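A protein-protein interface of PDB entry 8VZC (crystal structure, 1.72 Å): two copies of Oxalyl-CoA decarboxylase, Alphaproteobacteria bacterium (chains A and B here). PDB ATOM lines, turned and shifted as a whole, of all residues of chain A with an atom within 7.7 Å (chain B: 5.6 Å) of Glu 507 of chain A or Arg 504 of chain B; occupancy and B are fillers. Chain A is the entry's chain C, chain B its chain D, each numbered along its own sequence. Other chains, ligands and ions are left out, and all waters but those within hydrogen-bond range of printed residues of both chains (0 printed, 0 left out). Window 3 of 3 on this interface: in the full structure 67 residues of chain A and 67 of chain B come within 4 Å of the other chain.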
ATOM      1  N   PHE A 458      -4.483  26.882  23.029  1.00  0.00           N
ATOM      2  CA  PHE A 458      -4.406  26.111  24.269  1.00  0.00           C
ATOM      3  C   PHE A 458      -3.008  26.204  24.872  1.00  0.00           C
ATOM      4  O   PHE A 458      -2.847  26.198  26.099  1.00  0.00           O
ATOM      5  CB  PHE A 458      -4.774  24.657  24.011  1.00  0.00           C
ATOM      6  CG  PHE A 458      -4.954  23.850  25.280  1.00  0.00           C
ATOM      7  CD1 PHE A 458      -3.862  23.271  25.915  1.00  0.00           C
ATOM      8  CD2 PHE A 458      -6.205  23.693  25.817  1.00  0.00           C
ATOM      9  CE1 PHE A 458      -4.034  22.523  27.110  1.00  0.00           C
ATOM     10  CE2 PHE A 458      -6.390  22.956  26.986  1.00  0.00           C
ATOM     11  CZ  PHE A 458      -5.303  22.372  27.625  1.00  0.00           C
ATOM     12  N   ARG A 501      -8.728  12.861  17.774  1.00  0.00           N
ATOM     13  CA  ARG A 501      -8.520  12.808  19.218  1.00  0.00           C
ATOM     14  C   ARG A 501      -7.937  14.155  19.643  1.00  0.00           C
ATOM     15  O   ARG A 501      -6.767  14.269  20.042  1.00  0.00           O
ATOM     16  CB  ARG A 501      -7.610  11.593  19.589  1.00  0.00           C
ATOM     17  CG  ARG A 501      -8.170  10.199  19.189  1.00  0.00           C
ATOM     18  CD  ARG A 501      -9.326   9.767  20.078  1.00  0.00           C
ATOM     19  NE  ARG A 501      -8.891   9.603  21.455  1.00  0.00           N
ATOM     20  CZ  ARG A 501      -8.638   8.438  22.024  1.00  0.00           C
ATOM     21  NH1 ARG A 501      -8.768   7.302  21.358  1.00  0.00           N
ATOM     22  NH2 ARG A 501      -8.243   8.409  23.295  1.00  0.00           N
ATOM     23  N   TYR A 502      -8.784  15.194  19.521  1.00  0.00           N
ATOM     24  CA  TYR A 502      -8.369  16.563  19.805  1.00  0.00           C
ATOM     25  C   TYR A 502      -7.827  16.694  21.213  1.00  0.00           C
ATOM     26  O   TYR A 502      -6.971  17.548  21.480  1.00  0.00           O
ATOM     27  CB  TYR A 502      -9.543  17.534  19.636  1.00  0.00           C
ATOM     28  CG  TYR A 502     -10.030  17.748  18.221  1.00  0.00           C
ATOM     29  CD1 TYR A 502      -9.320  18.543  17.324  1.00  0.00           C
ATOM     30  CD2 TYR A 502     -11.213  17.165  17.783  1.00  0.00           C
ATOM     31  CE1 TYR A 502      -9.782  18.759  16.025  1.00  0.00           C
ATOM     32  CE2 TYR A 502     -11.690  17.382  16.491  1.00  0.00           C
ATOM     33  CZ  TYR A 502     -10.968  18.154  15.618  1.00  0.00           C
ATOM     34  OH  TYR A 502     -11.467  18.321  14.348  1.00  0.00           O
ATOM     35  N   GLU A 503      -8.337  15.884  22.142  1.00  0.00           N
ATOM     36  CA  GLU A 503      -7.881  16.044  23.511  1.00  0.00           C
ATOM     37  C   GLU A 503      -6.384  15.783  23.661  1.00  0.00           C
ATOM     38  O   GLU A 503      -5.787  16.261  24.628  1.00  0.00           O
ATOM     39  CB  GLU A 503      -8.702  15.142  24.449  1.00  0.00           C
ATOM     40  CG  GLU A 503      -8.267  13.672  24.460  1.00  0.00           C
ATOM     41  CD  GLU A 503      -8.628  12.878  23.213  1.00  0.00           C
ATOM     42  OE1 GLU A 503      -9.342  13.390  22.301  1.00  0.00           O
ATOM     43  OE2 GLU A 503      -8.154  11.718  23.132  1.00  0.00           O
ATOM     44  N   ARG A 504      -5.736  15.083  22.717  1.00  0.00           N
ATOM     45  CA  ARG A 504      -4.288  14.913  22.850  1.00  0.00           C
ATOM     46  C   ARG A 504      -3.532  16.224  22.687  1.00  0.00           C
ATOM     47  O   ARG A 504      -2.350  16.294  23.063  1.00  0.00           O
ATOM     48  CB  ARG A 504      -3.764  13.870  21.853  1.00  0.00           C
ATOM     49  CG  ARG A 504      -4.366  12.520  22.115  1.00  0.00           C
ATOM     50  CD  ARG A 504      -3.898  11.436  21.149  1.00  0.00           C
ATOM     51  NE  ARG A 504      -4.451  10.155  21.574  1.00  0.00           N
ATOM     52  CZ  ARG A 504      -4.703   9.128  20.774  1.00  0.00           C
ATOM     53  NH1 ARG A 504      -4.450   9.183  19.471  1.00  0.00           N
ATOM     54  NH2 ARG A 504      -5.236   8.023  21.293  1.00  0.00           N
ATOM     55  N   ILE A 505      -4.176  17.255  22.128  1.00  0.00           N
ATOM     56  CA  ILE A 505      -3.543  18.568  22.064  1.00  0.00           C
ATOM     57  C   ILE A 505      -3.317  19.109  23.480  1.00  0.00           C
ATOM     58  O   ILE A 505      -2.285  19.735  23.775  1.00  0.00           O
ATOM     59  CB  ILE A 505      -4.385  19.522  21.197  1.00  0.00           C
ATOM     60  CG1 ILE A 505      -4.413  19.030  19.738  1.00  0.00           C
ATOM     61  CG2 ILE A 505      -3.855  20.953  21.288  1.00  0.00           C
ATOM     62  CD1 ILE A 505      -5.311  19.865  18.840  1.00  0.00           C
ATOM     63  N   ALA A 506      -4.247  18.847  24.392  1.00  0.00           N
ATOM     64  CA  ALA A 506      -4.001  19.259  25.768  1.00  0.00           C
ATOM     65  C   ALA A 506      -2.710  18.658  26.278  1.00  0.00           C
ATOM     66  O   ALA A 506      -1.955  19.308  27.014  1.00  0.00           O
ATOM     67  CB  ALA A 506      -5.163  18.845  26.679  1.00  0.00           C
ATOM     68  N   GLU A 507      -2.466  17.395  25.926  1.00  0.00           N
ATOM     69  CA  GLU A 507      -1.340  16.661  26.462  1.00  0.00           C
ATOM     70  C   GLU A 507      -0.038  17.125  25.850  1.00  0.00           C
ATOM     71  O   GLU A 507       1.023  16.895  26.430  1.00  0.00           O
ATOM     72  CB  GLU A 507      -1.548  15.161  26.237  1.00  0.00           C
ATOM     73  CG  GLU A 507      -2.755  14.609  27.032  1.00  0.00           C
ATOM     74  CD  GLU A 507      -3.033  13.140  26.819  1.00  0.00           C
ATOM     75  OE1 GLU A 507      -2.586  12.580  25.801  1.00  0.00           O
ATOM     76  OE2 GLU A 507      -3.727  12.549  27.680  1.00  0.00           O
ATOM     77  N   ALA A 508      -0.101  17.797  24.698  1.00  0.00           N
ATOM     78  CA  ALA A 508       1.092  18.425  24.160  1.00  0.00           C
ATOM     79  C   ALA A 508       1.596  19.556  25.045  1.00  0.00           C
ATOM     80  O   ALA A 508       2.779  19.905  24.978  1.00  0.00           O
ATOM     81  CB  ALA A 508       0.793  18.976  22.759  1.00  0.00           C
ATOM     82  N   PHE A 509       0.722  20.147  25.865  1.00  0.00           N
ATOM     83  CA  PHE A 509       1.033  21.398  26.547  1.00  0.00           C
ATOM     84  C   PHE A 509       0.874  21.297  28.061  1.00  0.00           C
ATOM     85  O   PHE A 509       0.762  22.328  28.742  1.00  0.00           O
ATOM     86  CB  PHE A 509       0.164  22.510  25.972  1.00  0.00           C
ATOM     87  CG  PHE A 509       0.344  22.685  24.489  1.00  0.00           C
ATOM     88  CD1 PHE A 509       1.612  22.840  23.949  1.00  0.00           C
ATOM     89  CD2 PHE A 509      -0.743  22.663  23.635  1.00  0.00           C
ATOM     90  CE1 PHE A 509       1.791  22.999  22.568  1.00  0.00           C
ATOM     91  CE2 PHE A 509      -0.572  22.812  22.226  1.00  0.00           C
ATOM     92  CZ  PHE A 509       0.698  22.980  21.707  1.00  0.00           C
ATOM     93  N   GLY A 510       0.852  20.085  28.593  1.00  0.00           N
ATOM     94  CA  GLY A 510       0.769  19.890  30.030  1.00  0.00           C
ATOM     95  C   GLY A 510      -0.625  19.941  30.598  1.00  0.00           C
ATOM     96  O   GLY A 510      -0.777  19.894  31.829  1.00  0.00           O
ATOM     97  N   GLY A 511      -1.653  20.053  29.750  1.00  0.00           N
ATOM     98  CA  GLY A 511      -3.032  19.975  30.205  1.00  0.00           C
ATOM     99  C   GLY A 511      -3.540  18.542  30.284  1.00  0.00           C
ATOM    100  O   GLY A 511      -2.852  17.576  29.949  1.00  0.00           O
ATOM    101  N   ALA A 512      -4.778  18.406  30.751  1.00  0.00           N
ATOM    102  CA  ALA A 512      -5.410  17.102  30.877  1.00  0.00           C
ATOM    103  C   ALA A 512      -6.342  16.899  29.698  1.00  0.00           C
ATOM    104  O   ALA A 512      -7.130  17.787  29.375  1.00  0.00           O
ATOM    105  CB  ALA A 512      -6.187  16.979  32.188  1.00  0.00           C
ATOM    106  N   GLY A 513      -6.270  15.727  29.075  1.00  0.00           N
ATOM    107  CA  GLY A 513      -7.142  15.372  27.965  1.00  0.00           C
ATOM    108  C   GLY A 513      -8.082  14.238  28.336  1.00  0.00           C
ATOM    109  O   GLY A 513      -7.682  13.273  28.997  1.00  0.00           O
ATOM    110  N   PHE A 514      -9.330  14.357  27.900  1.00  0.00           N
ATOM    111  CA  PHE A 514     -10.343  13.341  28.147  1.00  0.00           C
ATOM    112  C   PHE A 514     -11.118  13.089  26.862  1.00  0.00           C
ATOM    113  O   PHE A 514     -11.505  14.034  26.168  1.00  0.00           O
ATOM    114  CB  PHE A 514     -11.305  13.773  29.274  1.00  0.00           C
ATOM    115  CG  PHE A 514     -10.595  14.185  30.530  1.00  0.00           C
ATOM    116  CD1 PHE A 514     -10.199  15.510  30.708  1.00  0.00           C
ATOM    117  CD2 PHE A 514     -10.317  13.242  31.540  1.00  0.00           C
ATOM    118  CE1 PHE A 514      -9.544  15.885  31.845  1.00  0.00           C
ATOM    119  CE2 PHE A 514      -9.645  13.607  32.685  1.00  0.00           C
ATOM    120  CZ  PHE A 514      -9.264  14.946  32.846  1.00  0.00           C
ATOM    121  N   PRO A 535      -5.511  23.778  32.598  1.00  0.00           N
ATOM    122  CA  PRO A 535      -6.406  23.721  31.435  1.00  0.00           C
ATOM    123  C   PRO A 535      -6.670  22.291  30.985  1.00  0.00           C
ATOM    124  O   PRO A 535      -5.874  21.378  31.229  1.00  0.00           O
ATOM    125  CB  PRO A 535      -5.636  24.495  30.365  1.00  0.00           C
ATOM    126  CG  PRO A 535      -4.161  24.234  30.736  1.00  0.00           C
ATOM    127  CD  PRO A 535      -4.162  24.278  32.259  1.00  0.00           C
ATOM    128  N   ILE A 537      -8.992  19.679  27.926  1.00  0.00           N
ATOM    129  CA  ILE A 537      -9.872  19.439  26.796  1.00  0.00           C
ATOM    130  C   ILE A 537     -10.673  18.166  27.050  1.00  0.00           C
ATOM    131  O   ILE A 537     -10.103  17.097  27.306  1.00  0.00           O
ATOM    132  CB  ILE A 537      -9.079  19.330  25.480  1.00  0.00           C
ATOM    133  CG1 ILE A 537      -8.375  20.651  25.196  1.00  0.00           C
ATOM    134  CG2 ILE A 537     -10.009  18.907  24.329  1.00  0.00           C
ATOM    135  CD1 ILE A 537      -7.586  20.685  23.821  1.00  0.00           C
ATOM    136  N   ARG B 501       5.313  19.387  23.922  1.00  0.00           N
ATOM    137  CA  ARG B 501       5.393  18.131  23.190  1.00  0.00           C
ATOM    138  C   ARG B 501       4.512  18.239  21.948  1.00  0.00           C
ATOM    139  O   ARG B 501       3.496  17.555  21.806  1.00  0.00           O
ATOM    140  CB  ARG B 501       4.981  16.942  24.116  1.00  0.00           C
ATOM    141  CG  ARG B 501       5.933  16.725  25.283  1.00  0.00           C
ATOM    142  CD  ARG B 501       7.318  16.279  24.844  1.00  0.00           C
ATOM    143  NE  ARG B 501       7.353  14.903  24.343  1.00  0.00           N
ATOM    144  CZ  ARG B 501       7.572  13.827  25.092  1.00  0.00           C
ATOM    145  NH1 ARG B 501       7.856  13.921  26.390  1.00  0.00           N
ATOM    146  NH2 ARG B 501       7.473  12.616  24.541  1.00  0.00           N
ATOM    147  N   TYR B 502       4.926  19.122  21.023  1.00  0.00           N
ATOM    148  CA  TYR B 502       4.119  19.402  19.841  1.00  0.00           C
ATOM    149  C   TYR B 502       3.808  18.149  19.037  1.00  0.00           C
ATOM    150  O   TYR B 502       2.787  18.102  18.341  1.00  0.00           O
ATOM    151  CB  TYR B 502       4.845  20.383  18.922  1.00  0.00           C
ATOM    152  CG  TYR B 502       4.929  21.789  19.434  1.00  0.00           C
ATOM    153  CD1 TYR B 502       3.803  22.614  19.462  1.00  0.00           C
ATOM    154  CD2 TYR B 502       6.139  22.298  19.878  1.00  0.00           C
ATOM    155  CE1 TYR B 502       3.874  23.917  19.931  1.00  0.00           C
ATOM    156  CE2 TYR B 502       6.220  23.578  20.354  1.00  0.00           C
ATOM    157  CZ  TYR B 502       5.086  24.391  20.371  1.00  0.00           C
ATOM    158  OH  TYR B 502       5.190  25.672  20.839  1.00  0.00           O
ATOM    159  N   GLU B 503       4.695  17.150  19.064  1.00  0.00           N
ATOM    160  CA  GLU B 503       4.476  15.965  18.243  1.00  0.00           C
ATOM    161  C   GLU B 503       3.216  15.215  18.657  1.00  0.00           C
ATOM    162  O   GLU B 503       2.678  14.438  17.864  1.00  0.00           O
ATOM    163  CB  GLU B 503       5.718  15.051  18.283  1.00  0.00           C
ATOM    164  CG  GLU B 503       5.880  14.194  19.531  1.00  0.00           C
ATOM    165  CD  GLU B 503       6.233  14.961  20.805  1.00  0.00           C
ATOM    166  OE1 GLU B 503       6.449  16.185  20.755  1.00  0.00           O
ATOM    167  OE2 GLU B 503       6.305  14.301  21.885  1.00  0.00           O
ATOM    168  N   ARG B 504       2.717  15.445  19.871  1.00  0.00           N
ATOM    169  CA  ARG B 504       1.460  14.808  20.256  1.00  0.00           C
ATOM    170  C   ARG B 504       0.282  15.320  19.443  1.00  0.00           C
ATOM    171  O   ARG B 504      -0.748  14.643  19.382  1.00  0.00           O
ATOM    172  CB  ARG B 504       1.227  14.996  21.753  1.00  0.00           C
ATOM    173  CG  ARG B 504       2.297  14.268  22.546  1.00  0.00           C
ATOM    174  CD  ARG B 504       2.146  14.482  24.066  1.00  0.00           C
ATOM    175  NE  ARG B 504       3.106  13.645  24.768  1.00  0.00           N
ATOM    176  CZ  ARG B 504       3.514  13.843  26.014  1.00  0.00           C
ATOM    177  NH1 ARG B 504       3.104  14.886  26.720  1.00  0.00           N
ATOM    178  NH2 ARG B 504       4.352  12.968  26.568  1.00  0.00           N
ATOM    179  N   ILE B 505       0.421  16.472  18.783  1.00  0.00           N
ATOM    180  CA  ILE B 505      -0.625  16.918  17.870  1.00  0.00           C
ATOM    181  C   ILE B 505      -0.747  15.947  16.697  1.00  0.00           C
ATOM    182  O   ILE B 505      -1.855  15.648  16.227  1.00  0.00           O
ATOM    183  CB  ILE B 505      -0.342  18.362  17.420  1.00  0.00           C
ATOM    184  CG1 ILE B 505      -0.368  19.292  18.641  1.00  0.00           C
ATOM    185  CG2 ILE B 505      -1.323  18.827  16.350  1.00  0.00           C
ATOM    186  CD1 ILE B 505       0.199  20.681  18.349  1.00  0.00           C
ATOM    187  N   ALA B 506       0.385  15.434  16.204  1.00  0.00           N
ATOM    188  CA  ALA B 506       0.317  14.423  15.155  1.00  0.00           C
ATOM    189  C   ALA B 506      -0.548  13.254  15.588  1.00  0.00           C
ATOM    190  O   ALA B 506      -1.365  12.749  14.809  1.00  0.00           O
ATOM    191  CB  ALA B 506       1.718  13.941  14.784  1.00  0.00           C
ATOM    192  N   GLU B 507      -0.392  12.819  16.838  1.00  0.00           N
ATOM    193  CA  GLU B 507      -1.120  11.662  17.320  1.00  0.00           C
ATOM    194  C   GLU B 507      -2.597  11.955  17.485  1.00  0.00           C
ATOM    195  O   GLU B 507      -3.400  11.020  17.529  1.00  0.00           O
ATOM    196  CB  GLU B 507      -0.491  11.184  18.637  1.00  0.00           C
ATOM    197  CG  GLU B 507       0.992  10.812  18.407  1.00  0.00           C
ATOM    198  CD  GLU B 507       1.719  10.356  19.649  1.00  0.00           C
ATOM    199  OE1 GLU B 507       1.362  10.797  20.750  1.00  0.00           O
ATOM    200  OE2 GLU B 507       2.666   9.550  19.523  1.00  0.00           O
ATOM    201  N   ALA B 508      -2.974  13.229  17.586  1.00  0.00           N
ATOM    202  CA  ALA B 508      -4.393  13.556  17.606  1.00  0.00           C
ATOM    203  C   ALA B 508      -5.058  13.165  16.296  1.00  0.00           C
ATOM    204  O   ALA B 508      -6.231  12.792  16.284  1.00  0.00           O
ATOM    205  CB  ALA B 508      -4.600  15.049  17.900  1.00  0.00           C
ATOM    206  N   GLY B 513       4.265  10.871  15.693  1.00  0.00           N
ATOM    207  CA  GLY B 513       4.960  11.915  16.426  1.00  0.00           C
ATOM    208  C   GLY B 513       6.270  11.376  16.971  1.00  0.00           C
ATOM    209  O   GLY B 513       6.321  10.245  17.455  1.00  0.00           O
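The backbone carbonyl oxygen (O) of Ala 508 of chain B lies within hydrogen-bond range of the backbone NH (N) of Arg 501 of chain A, 2.9 Å away.
The guanidinium group of Arg 504 of chain A lies within hydrogen-bond range of the backbone carbonyl oxygen of Glu 507 of chain B, at 2.9 Å.
The backbone carbonyl oxygen (O) of Ala 508 of chain A lies within hydrogen-bond range of the backbone NH (N) of Arg 501 of chain B.
The backbone carbonyl oxygen (O) of Glu 507 of chain A lies within hydrogen-bond range of the guanidinium group (NH1) of Arg 504 of chain B (2.9 Å).
OE2 of Glu 503 of chain B is in salt-bridge range of NE of Arg 501 of chain B, 2.7 Å away.
OE2 of Glu 503 of chain A lies within salt-bridge range of NE of Arg 501 of chain A, 2.8 Å away.
Among the printed residues, pairs that only touch across the chains: Phe 509 of chain A with Tyr 502 of chain B and Arg 504 of chain A with Arg 504 of chain B.
Glu 507 of chain A touches just one residue of chain B: Arg 504 (2.9 Å).
Arg 504 of chain B touches just these residues of chain A: Arg 504 and Glu 507.
Of the printed residues of chain B, Ala 508 of chain A touches Arg 501.
Of the printed residues of chain B, Arg 504 of chain A touches Arg 504 and Glu 507.
Glu 503 of chain A touches none of the printed residues of chain B.
Ile 505 of chain B touches none of the printed residues of chain A.
The nearest printed residue of chain A that does not touch Ala 508 of chain B is Arg 504 of chain A (4.1 Å).
Printed residues of chain B that touch a printed residue of chain A: Arg 501, Tyr 502, Arg 504, Glu 507 and Ala 508.
Of the 17 printed residues of chain A, 5 touch a printed residue of chain B.
Hydrophobic or aromatic side chains of chain A within 4 Å of the printed part of chain B: Ala 508 and Phe 509.
Arg 501 of chain A touches Ala 508 of chain B, and with the chains exchanged Ala 508 of chain A touches Arg 501 of chain B.
Arg 504 of chain A touches its own counterpart, Arg 504 of chain B.
Arg 504 of chain A touches Glu 507 of chain B, and with the chains exchanged Glu 507 of chain A touches Arg 504 of chain B.
Positions printed for both chains: 501, 502, 503, 504, 505, 506, 507, 508 and 513.
Of the 6 pairs that touch across the chains among the printed residues, 5 have their exchanged pair printed and touching as well.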
